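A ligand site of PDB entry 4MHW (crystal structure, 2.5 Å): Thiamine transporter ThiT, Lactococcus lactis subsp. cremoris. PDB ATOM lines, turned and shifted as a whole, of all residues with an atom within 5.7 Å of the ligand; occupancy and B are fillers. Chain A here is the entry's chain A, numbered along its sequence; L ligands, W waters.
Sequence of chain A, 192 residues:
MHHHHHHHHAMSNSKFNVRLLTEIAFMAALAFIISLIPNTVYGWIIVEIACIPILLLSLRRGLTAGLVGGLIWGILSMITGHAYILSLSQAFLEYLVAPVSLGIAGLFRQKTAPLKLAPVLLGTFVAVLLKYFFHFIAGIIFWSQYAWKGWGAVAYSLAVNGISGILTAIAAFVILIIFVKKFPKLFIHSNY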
ATOM      1  N   TRP A  44     -15.149   2.528 -22.166  1.00  0.00           N
ATOM      2  CA  TRP A  44     -16.202   2.341 -21.163  1.00  0.00           C
ATOM      3  C   TRP A  44     -15.757   2.693 -19.746  1.00  0.00           C
ATOM      4  O   TRP A  44     -16.376   2.258 -18.812  1.00  0.00           O
ATOM      5  CB  TRP A  44     -16.788   0.919 -21.234  1.00  0.00           C
ATOM      6  CG  TRP A  44     -18.237   0.926 -21.702  1.00  0.00           C
ATOM      7  CD1 TRP A  44     -18.716   0.490 -22.908  1.00  0.00           C
ATOM      8  CD2 TRP A  44     -19.362   1.425 -20.975  1.00  0.00           C
ATOM      9  NE1 TRP A  44     -20.078   0.684 -22.960  1.00  0.00           N
ATOM     10  CE2 TRP A  44     -20.496   1.259 -21.793  1.00  0.00           C
ATOM     11  CE3 TRP A  44     -19.530   2.006 -19.704  1.00  0.00           C
ATOM     12  CZ2 TRP A  44     -21.783   1.636 -21.380  1.00  0.00           C
ATOM     13  CZ3 TRP A  44     -20.804   2.383 -19.296  1.00  0.00           C
ATOM     14  CH2 TRP A  44     -21.908   2.197 -20.135  1.00  0.00           C
ATOM     15  N   ILE A  46     -15.787   5.407 -17.032  1.00  0.00           N
ATOM     16  CA  ILE A  46     -16.590   6.588 -16.820  1.00  0.00           C
ATOM     17  C   ILE A  46     -16.429   7.079 -15.415  1.00  0.00           C
ATOM     18  O   ILE A  46     -15.955   6.355 -14.526  1.00  0.00           O
ATOM     19  CB  ILE A  46     -18.050   6.281 -17.114  1.00  0.00           C
ATOM     20  CG1 ILE A  46     -18.568   5.146 -16.232  1.00  0.00           C
ATOM     21  CG2 ILE A  46     -18.188   5.883 -18.558  1.00  0.00           C
ATOM     22  CD1 ILE A  46     -20.027   4.901 -16.422  1.00  0.00           C
ATOM     23  N   GLU A  48     -19.024   8.135 -12.882  1.00  0.00           N
ATOM     24  CA  GLU A  48     -20.499   8.154 -12.831  1.00  0.00           C
ATOM     25  C   GLU A  48     -21.085   9.071 -11.731  1.00  0.00           C
ATOM     26  O   GLU A  48     -21.728   8.599 -10.821  1.00  0.00           O
ATOM     27  CB  GLU A  48     -21.124   6.741 -12.743  1.00  0.00           C
ATOM     28  CG  GLU A  48     -22.530   6.729 -13.379  1.00  0.00           C
ATOM     29  CD  GLU A  48     -23.232   5.386 -13.257  1.00  0.00           C
ATOM     30  OE1 GLU A  48     -22.772   4.599 -12.444  1.00  0.00           O
ATOM     31  OE2 GLU A  48     -24.232   5.118 -13.976  1.00  0.00           O
ATOM     32  N   TYR A  84     -27.613   1.271 -22.407  1.00  0.00           N
ATOM     33  CA  TYR A  84     -26.995   0.364 -23.381  1.00  0.00           C
ATOM     34  C   TYR A  84     -27.354  -1.061 -22.985  1.00  0.00           C
ATOM     35  O   TYR A  84     -26.893  -1.594 -21.947  1.00  0.00           O
ATOM     36  CB  TYR A  84     -25.470   0.553 -23.418  1.00  0.00           C
ATOM     37  CG  TYR A  84     -25.091   2.006 -23.539  1.00  0.00           C
ATOM     38  CD1 TYR A  84     -24.949   2.819 -22.409  1.00  0.00           C
ATOM     39  CD2 TYR A  84     -24.918   2.597 -24.778  1.00  0.00           C
ATOM     40  CE1 TYR A  84     -24.632   4.164 -22.531  1.00  0.00           C
ATOM     41  CE2 TYR A  84     -24.588   3.921 -24.907  1.00  0.00           C
ATOM     42  CZ  TYR A  84     -24.452   4.706 -23.793  1.00  0.00           C
ATOM     43  OH  TYR A  84     -24.137   6.024 -23.962  1.00  0.00           O
ATOM     44  N   GLN A  90     -29.056  -8.699 -19.252  1.00  0.00           N
ATOM     45  CA  GLN A  90     -27.986  -7.709 -19.095  1.00  0.00           C
ATOM     46  C   GLN A  90     -28.600  -6.355 -18.719  1.00  0.00           C
ATOM     47  O   GLN A  90     -28.015  -5.598 -17.940  1.00  0.00           O
ATOM     48  CB  GLN A  90     -27.120  -7.618 -20.356  1.00  0.00           C
ATOM     49  CG  GLN A  90     -26.137  -6.450 -20.393  1.00  0.00           C
ATOM     50  CD  GLN A  90     -26.803  -5.143 -20.827  1.00  0.00           C
ATOM     51  OE1 GLN A  90     -27.813  -5.161 -21.535  1.00  0.00           O
ATOM     52  NE2 GLN A  90     -26.242  -4.010 -20.377  1.00  0.00           N
ATOM     53  N   GLU A  94     -27.679  -4.640 -15.091  1.00  0.00           N
ATOM     54  CA  GLU A  94     -26.978  -3.346 -15.095  1.00  0.00           C
ATOM     55  C   GLU A  94     -27.845  -2.086 -14.974  1.00  0.00           C
ATOM     56  O   GLU A  94     -27.332  -0.987 -14.714  1.00  0.00           O
ATOM     57  CB  GLU A  94     -26.124  -3.194 -16.369  1.00  0.00           C
ATOM     58  CG  GLU A  94     -25.086  -4.323 -16.558  1.00  0.00           C
ATOM     59  CD  GLU A  94     -23.970  -3.894 -17.473  1.00  0.00           C
ATOM     60  OE1 GLU A  94     -23.095  -3.189 -16.928  1.00  0.00           O
ATOM     61  OE2 GLU A  94     -23.978  -4.232 -18.710  1.00  0.00           O
ATOM     62  N   TYR A  95     -29.150  -2.222 -15.197  1.00  0.00           N
ATOM     63  CA  TYR A  95     -30.034  -1.058 -15.123  1.00  0.00           C
ATOM     64  C   TYR A  95     -31.218  -1.269 -14.148  1.00  0.00           C
ATOM     65  O   TYR A  95     -32.112  -0.436 -14.076  1.00  0.00           O
ATOM     66  CB  TYR A  95     -30.521  -0.636 -16.532  1.00  0.00           C
ATOM     67  CG  TYR A  95     -29.451   0.032 -17.410  1.00  0.00           C
ATOM     68  CD1 TYR A  95     -29.188   1.401 -17.313  1.00  0.00           C
ATOM     69  CD2 TYR A  95     -28.698  -0.724 -18.323  1.00  0.00           C
ATOM     70  CE1 TYR A  95     -28.220   2.015 -18.098  1.00  0.00           C
ATOM     71  CE2 TYR A  95     -27.721  -0.119 -19.126  1.00  0.00           C
ATOM     72  CZ  TYR A  95     -27.470   1.259 -19.002  1.00  0.00           C
ATOM     73  OH  TYR A  95     -26.506   1.873 -19.799  1.00  0.00           O
ATOM     74  N   LYS A 131     -22.085  -1.525  -6.713  1.00  0.00           N
ATOM     75  CA  LYS A 131     -22.609  -1.288  -8.042  1.00  0.00           C
ATOM     76  C   LYS A 131     -21.634  -1.767  -9.112  1.00  0.00           C
ATOM     77  O   LYS A 131     -22.031  -2.403 -10.095  1.00  0.00           O
ATOM     78  CB  LYS A 131     -22.944   0.191  -8.236  1.00  0.00           C
ATOM     79  CG  LYS A 131     -23.681   0.481  -9.526  1.00  0.00           C
ATOM     80  CD  LYS A 131     -24.179   1.926  -9.609  1.00  0.00           C
ATOM     81  CE  LYS A 131     -25.076   2.134 -10.825  1.00  0.00           C
ATOM     82  NZ  LYS A 131     -24.350   2.394 -12.139  1.00  0.00           N
ATOM     83  N   TYR A 132     -20.353  -1.446  -8.933  1.00  0.00           N
ATOM     84  CA  TYR A 132     -19.381  -1.727  -9.970  1.00  0.00           C
ATOM     85  C   TYR A 132     -18.893  -3.180  -9.914  1.00  0.00           C
ATOM     86  O   TYR A 132     -18.291  -3.708 -10.850  1.00  0.00           O
ATOM     87  CB  TYR A 132     -18.283  -0.666  -9.961  1.00  0.00           C
ATOM     88  CG  TYR A 132     -18.718   0.456 -10.830  1.00  0.00           C
ATOM     89  CD1 TYR A 132     -19.502   1.474 -10.321  1.00  0.00           C
ATOM     90  CD2 TYR A 132     -18.432   0.454 -12.231  1.00  0.00           C
ATOM     91  CE1 TYR A 132     -19.993   2.526 -11.175  1.00  0.00           C
ATOM     92  CE2 TYR A 132     -18.879   1.495 -13.087  1.00  0.00           C
ATOM     93  CZ  TYR A 132     -19.679   2.510 -12.542  1.00  0.00           C
ATOM     94  OH  TYR A 132     -20.169   3.519 -13.355  1.00  0.00           O
ATOM     95  N   PHE A 134     -21.272  -5.363  -9.854  1.00  0.00           N
ATOM     96  CA  PHE A 134     -22.271  -5.940 -10.735  1.00  0.00           C
ATOM     97  C   PHE A 134     -21.846  -5.691 -12.189  1.00  0.00           C
ATOM     98  O   PHE A 134     -21.903  -6.580 -13.010  1.00  0.00           O
ATOM     99  CB  PHE A 134     -23.688  -5.452 -10.408  1.00  0.00           C
ATOM    100  CG  PHE A 134     -24.264  -6.062  -9.157  1.00  0.00           C
ATOM    101  CD1 PHE A 134     -24.435  -7.430  -9.045  1.00  0.00           C
ATOM    102  CD2 PHE A 134     -24.603  -5.253  -8.060  1.00  0.00           C
ATOM    103  CE1 PHE A 134     -24.949  -7.997  -7.851  1.00  0.00           C
ATOM    104  CE2 PHE A 134     -25.108  -5.819  -6.884  1.00  0.00           C
ATOM    105  CZ  PHE A 134     -25.275  -7.186  -6.782  1.00  0.00           C
ATOM    106  N   HIS A 135     -21.391  -4.478 -12.488  1.00  0.00           N
ATOM    107  CA  HIS A 135     -20.852  -4.173 -13.798  1.00  0.00           C
ATOM    108  C   HIS A 135     -19.672  -5.039 -14.213  1.00  0.00           C
ATOM    109  O   HIS A 135     -19.540  -5.425 -15.378  1.00  0.00           O
ATOM    110  CB  HIS A 135     -20.430  -2.729 -13.822  1.00  0.00           C
ATOM    111  CG  HIS A 135     -21.584  -1.800 -13.721  1.00  0.00           C
ATOM    112  ND1 HIS A 135     -22.663  -1.876 -14.552  1.00  0.00           N
ATOM    113  CD2 HIS A 135     -21.827  -0.764 -12.875  1.00  0.00           C
ATOM    114  CE1 HIS A 135     -23.523  -0.931 -14.249  1.00  0.00           C
ATOM    115  NE2 HIS A 135     -23.043  -0.240 -13.225  1.00  0.00           N
ATOM    116  N   PHE A 136     -18.804  -5.317 -13.258  1.00  0.00           N
ATOM    117  CA  PHE A 136     -17.639  -6.177 -13.471  1.00  0.00           C
ATOM    118  C   PHE A 136     -18.106  -7.588 -13.874  1.00  0.00           C
ATOM    119  O   PHE A 136     -17.559  -8.196 -14.796  1.00  0.00           O
ATOM    120  CB  PHE A 136     -16.805  -6.210 -12.164  1.00  0.00           C
ATOM    121  CG  PHE A 136     -15.883  -7.378 -12.056  1.00  0.00           C
ATOM    122  CD1 PHE A 136     -14.712  -7.454 -12.824  1.00  0.00           C
ATOM    123  CD2 PHE A 136     -16.169  -8.411 -11.161  1.00  0.00           C
ATOM    124  CE1 PHE A 136     -13.873  -8.550 -12.716  1.00  0.00           C
ATOM    125  CE2 PHE A 136     -15.321  -9.518 -11.050  1.00  0.00           C
ATOM    126  CZ  PHE A 136     -14.178  -9.592 -11.830  1.00  0.00           C
ATOM    127  N   ALA A 138     -21.124  -8.179 -15.111  1.00  0.00           N
ATOM    128  CA  ALA A 138     -21.714  -7.903 -16.412  1.00  0.00           C
ATOM    129  C   ALA A 138     -20.622  -7.844 -17.471  1.00  0.00           C
ATOM    130  O   ALA A 138     -20.778  -8.389 -18.558  1.00  0.00           O
ATOM    131  CB  ALA A 138     -22.485  -6.587 -16.397  1.00  0.00           C
ATOM    132  N   GLY A 139     -19.514  -7.178 -17.152  1.00  0.00           N
ATOM    133  CA  GLY A 139     -18.446  -6.955 -18.113  1.00  0.00           C
ATOM    134  C   GLY A 139     -17.835  -8.270 -18.598  1.00  0.00           C
ATOM    135  O   GLY A 139     -17.422  -8.406 -19.740  1.00  0.00           O
ATOM    136  N   ILE A 140     -17.803  -9.251 -17.719  1.00  0.00           N
ATOM    137  CA  ILE A 140     -17.263 -10.554 -18.070  1.00  0.00           C
ATOM    138  C   ILE A 140     -18.236 -11.270 -18.981  1.00  0.00           C
ATOM    139  O   ILE A 140     -17.830 -11.836 -19.999  1.00  0.00           O
ATOM    140  CB  ILE A 140     -16.994 -11.399 -16.820  1.00  0.00           C
ATOM    141  CG1 ILE A 140     -15.896 -10.753 -15.977  1.00  0.00           C
ATOM    142  CG2 ILE A 140     -16.643 -12.856 -17.191  1.00  0.00           C
ATOM    143  CD1 ILE A 140     -15.727 -11.336 -14.569  1.00  0.00           C
ATOM    144  N   TRP A 143     -19.706  -8.259 -22.268  1.00  0.00           N
ATOM    145  CA  TRP A 143     -18.914  -7.219 -22.920  1.00  0.00           C
ATOM    146  C   TRP A 143     -17.528  -7.623 -23.410  1.00  0.00           C
ATOM    147  O   TRP A 143     -16.755  -6.769 -23.850  1.00  0.00           O
ATOM    148  CB  TRP A 143     -18.755  -6.032 -21.968  1.00  0.00           C
ATOM    149  CG  TRP A 143     -20.061  -5.396 -21.646  1.00  0.00           C
ATOM    150  CD1 TRP A 143     -20.890  -5.673 -20.590  1.00  0.00           C
ATOM    151  CD2 TRP A 143     -20.715  -4.376 -22.412  1.00  0.00           C
ATOM    152  NE1 TRP A 143     -22.004  -4.874 -20.643  1.00  0.00           N
ATOM    153  CE2 TRP A 143     -21.924  -4.071 -21.747  1.00  0.00           C
ATOM    154  CE3 TRP A 143     -20.386  -3.694 -23.596  1.00  0.00           C
ATOM    155  CZ2 TRP A 143     -22.820  -3.105 -22.230  1.00  0.00           C
ATOM    156  CZ3 TRP A 143     -21.264  -2.730 -24.071  1.00  0.00           C
ATOM    157  CH2 TRP A 143     -22.472  -2.436 -23.384  1.00  0.00           C
ATOM    158  N   TYR A 156      -9.990  -7.662 -18.360  1.00  0.00           N
ATOM    159  CA  TYR A 156     -10.523  -6.518 -19.085  1.00  0.00           C
ATOM    160  C   TYR A 156     -11.636  -5.856 -18.265  1.00  0.00           C
ATOM    161  O   TYR A 156     -11.680  -4.630 -18.143  1.00  0.00           O
ATOM    162  CB  TYR A 156     -11.040  -6.960 -20.475  1.00  0.00           C
ATOM    163  CG  TYR A 156     -11.814  -5.886 -21.237  1.00  0.00           C
ATOM    164  CD1 TYR A 156     -11.220  -4.666 -21.549  1.00  0.00           C
ATOM    165  CD2 TYR A 156     -13.127  -6.088 -21.644  1.00  0.00           C
ATOM    166  CE1 TYR A 156     -11.921  -3.660 -22.238  1.00  0.00           C
ATOM    167  CE2 TYR A 156     -13.851  -5.071 -22.354  1.00  0.00           C
ATOM    168  CZ  TYR A 156     -13.220  -3.864 -22.628  1.00  0.00           C
ATOM    169  OH  TYR A 156     -13.862  -2.841 -23.300  1.00  0.00           O
ATOM    170  N   SER A 157     -12.524  -6.675 -17.711  1.00  0.00           N
ATOM    171  CA  SER A 157     -13.633  -6.141 -16.919  1.00  0.00           C
ATOM    172  C   SER A 157     -13.158  -5.532 -15.605  1.00  0.00           C
ATOM    173  O   SER A 157     -13.725  -4.546 -15.164  1.00  0.00           O
ATOM    174  CB  SER A 157     -14.648  -7.219 -16.604  1.00  0.00           C
ATOM    175  OG  SER A 157     -15.853  -6.592 -16.215  1.00  0.00           O
ATOM    176  N   VAL A 160     -11.554  -2.029 -16.511  1.00  0.00           N
ATOM    177  CA  VAL A 160     -12.566  -1.072 -16.960  1.00  0.00           C
ATOM    178  C   VAL A 160     -13.536  -0.700 -15.817  1.00  0.00           C
ATOM    179  O   VAL A 160     -13.874   0.458 -15.614  1.00  0.00           O
ATOM    180  CB  VAL A 160     -13.414  -1.632 -18.124  1.00  0.00           C
ATOM    181  CG1 VAL A 160     -14.608  -0.714 -18.395  1.00  0.00           C
ATOM    182  CG2 VAL A 160     -12.568  -1.769 -19.419  1.00  0.00           C
ATOM    183  N   ASN A 161     -14.016  -1.704 -15.098  1.00  0.00           N
ATOM    184  CA  ASN A 161     -14.966  -1.455 -14.042  1.00  0.00           C
ATOM    185  C   ASN A 161     -14.283  -1.114 -12.714  1.00  0.00           C
ATOM    186  O   ASN A 161     -14.812  -0.336 -11.928  1.00  0.00           O
ATOM    187  CB  ASN A 161     -15.943  -2.636 -13.969  1.00  0.00           C
ATOM    188  CG  ASN A 161     -16.820  -2.679 -15.191  1.00  0.00           C
ATOM    189  OD1 ASN A 161     -16.881  -3.685 -15.921  1.00  0.00           O
ATOM    190  ND2 ASN A 161     -17.463  -1.556 -15.460  1.00  0.00           N
HETATM  191  C1  LIG L   1     -16.163  -4.078 -19.871  1.00  0.00           C
HETATM  192  C2  LIG L   1     -21.408  -1.766 -19.128  1.00  0.00           C
HETATM  193  C3  LIG L   1     -20.415  -0.380 -17.151  1.00  0.00           C
HETATM  194  S1  LIG L   1     -21.074   0.840 -16.187  1.00  0.00           S
HETATM  195  C4  LIG L   1     -22.622   0.969 -16.759  1.00  0.00           C
HETATM  196  C5  LIG L   1     -22.688   0.027 -17.807  1.00  0.00           C
HETATM  197  C6  LIG L   1     -23.915  -0.205 -18.650  1.00  0.00           C
HETATM  198  C7  LIG L   1     -23.699   1.916 -16.268  1.00  0.00           C
HETATM  199  C8  LIG L   1     -23.281   3.369 -16.404  1.00  0.00           C
HETATM  200  O1  LIG L   1     -23.866   3.924 -17.553  1.00  0.00           O
HETATM  201  N1  LIG L   1     -18.000  -2.614 -20.492  1.00  0.00           N
HETATM  202  C9  LIG L   1     -17.563  -3.484 -19.640  1.00  0.00           C
HETATM  203  N2  LIG L   1     -18.309  -3.843 -18.583  1.00  0.00           N
HETATM  204  C10 LIG L   1     -19.518  -3.346 -18.325  1.00  0.00           C
HETATM  205  N3  LIG L   1     -20.244  -3.776 -17.153  1.00  0.00           N
HETATM  206  C11 LIG L   1     -20.033  -2.408 -19.263  1.00  0.00           C
HETATM  207  C12 LIG L   1     -19.239  -2.065 -20.376  1.00  0.00           C
HETATM  208  C13 LIG L   1     -21.471  -0.724 -18.022  1.00  0.00           C
HETATM  209  O   HOH W   1     -26.088   3.717 -14.906  1.00  0.00           O
HETATM  210  O   HOH W   2     -16.383  -3.005 -22.959  1.00  0.00           O
HETATM  211  O   HOH W   3     -23.084   7.048 -17.506  1.00  0.00           O
HETATM  212  O   HOH W   4     -26.022   5.038 -18.585  1.00  0.00           O
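OD1 of Asn 161 sits close to O of His 135, 3.2 Å away. OH of Tyr 95 is in hydrogen-bond range of N of Tyr 84 (2.9 Å). NE1 of Trp 143 sits at hydrogen-bond distance from OE2 of Glu 94 (2.8 Å). The side-chain amide oxygen (OD1) of Asn 161 is in hydrogen-bond range of the side-chain hydroxyl (OG) of Ser 157 (3.1 Å). OE1 of Glu 94 is in hydrogen-bond range of ND1 of His 135 (2.7 Å). The side-chain hydroxyl of Tyr 132 is in hydrogen-bond range of the side-chain carboxylate of Glu 48, 3.0 Å away. The side-chain carboxylate of Glu 94 sits at hydrogen-bond distance from the side-chain amide nitrogen of Gln 90 (2.8 Å). The side-chain carboxylate of Glu 48 lies within salt-bridge range of the side-chain amino group of Lys 131, at 2.7 Å.
N of Gly 139 lies close to N3 of the ligand. Trp 44 touches the ligand (CH2 to C5, 3.3 Å). CD1 of Ile 46 touches C8 of the ligand (3.6 Å). Glu 48 touches the ligand. OH of Tyr 95 touches C6 of the ligand, at 3.5 Å. Tyr 132 touches the ligand. CB of Ala 138 touches N3 of the ligand (3.7 Å). Trp 143 touches the ligand. Tyr 156 touches the ligand (CE2 to C1, 3.5 Å). CG1 of Val 160 touches C1 of the ligand (3.99 Å). Hydrophobic or aromatic side chains that line the ligand: Trp 44, Ile 46, Tyr 95, Tyr 132, His 135, Ala 138, Trp 143, Tyr 156 and Val 160. Within 4 Å of the ligand: Trp 44, Ile 46, Glu 48, Glu 94, Tyr 95, Tyr 132, His 135, Ala 138, Gly 139, Trp 143, Tyr 156, Val 160 and Asn 161. The nearest printed residue that does not touch the ligand is Lys 131 (4.2 Å).
Water W4 lies within hydrogen-bond range of O1 of the ligand (2.6 Å) and OH of Tyr 95 (3.4 Å). Water W2 bridges the side-chain hydroxyl of Tyr 156 and a nitrogen (N1) of the ligand. Water W1 lies within hydrogen-bond range of OE2 of Glu 48 (2.5 Å) and O1 of the ligand (3.5 Å).
A nitrogen (N3) of the ligand is in hydrogen-bond range of the backbone carbonyl oxygen (O) of His 135 (2.5 Å). The side-chain carboxylate (OE1) of Glu 94 lies within hydrogen-bond range of a nitrogen (N3) of the ligand, 2.9 Å away. ND1 of His 135 lies close to S1 of the ligand (3.5 Å). N2 of the ligand sits close to OD1 of Asn 161 (3.0 Å).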
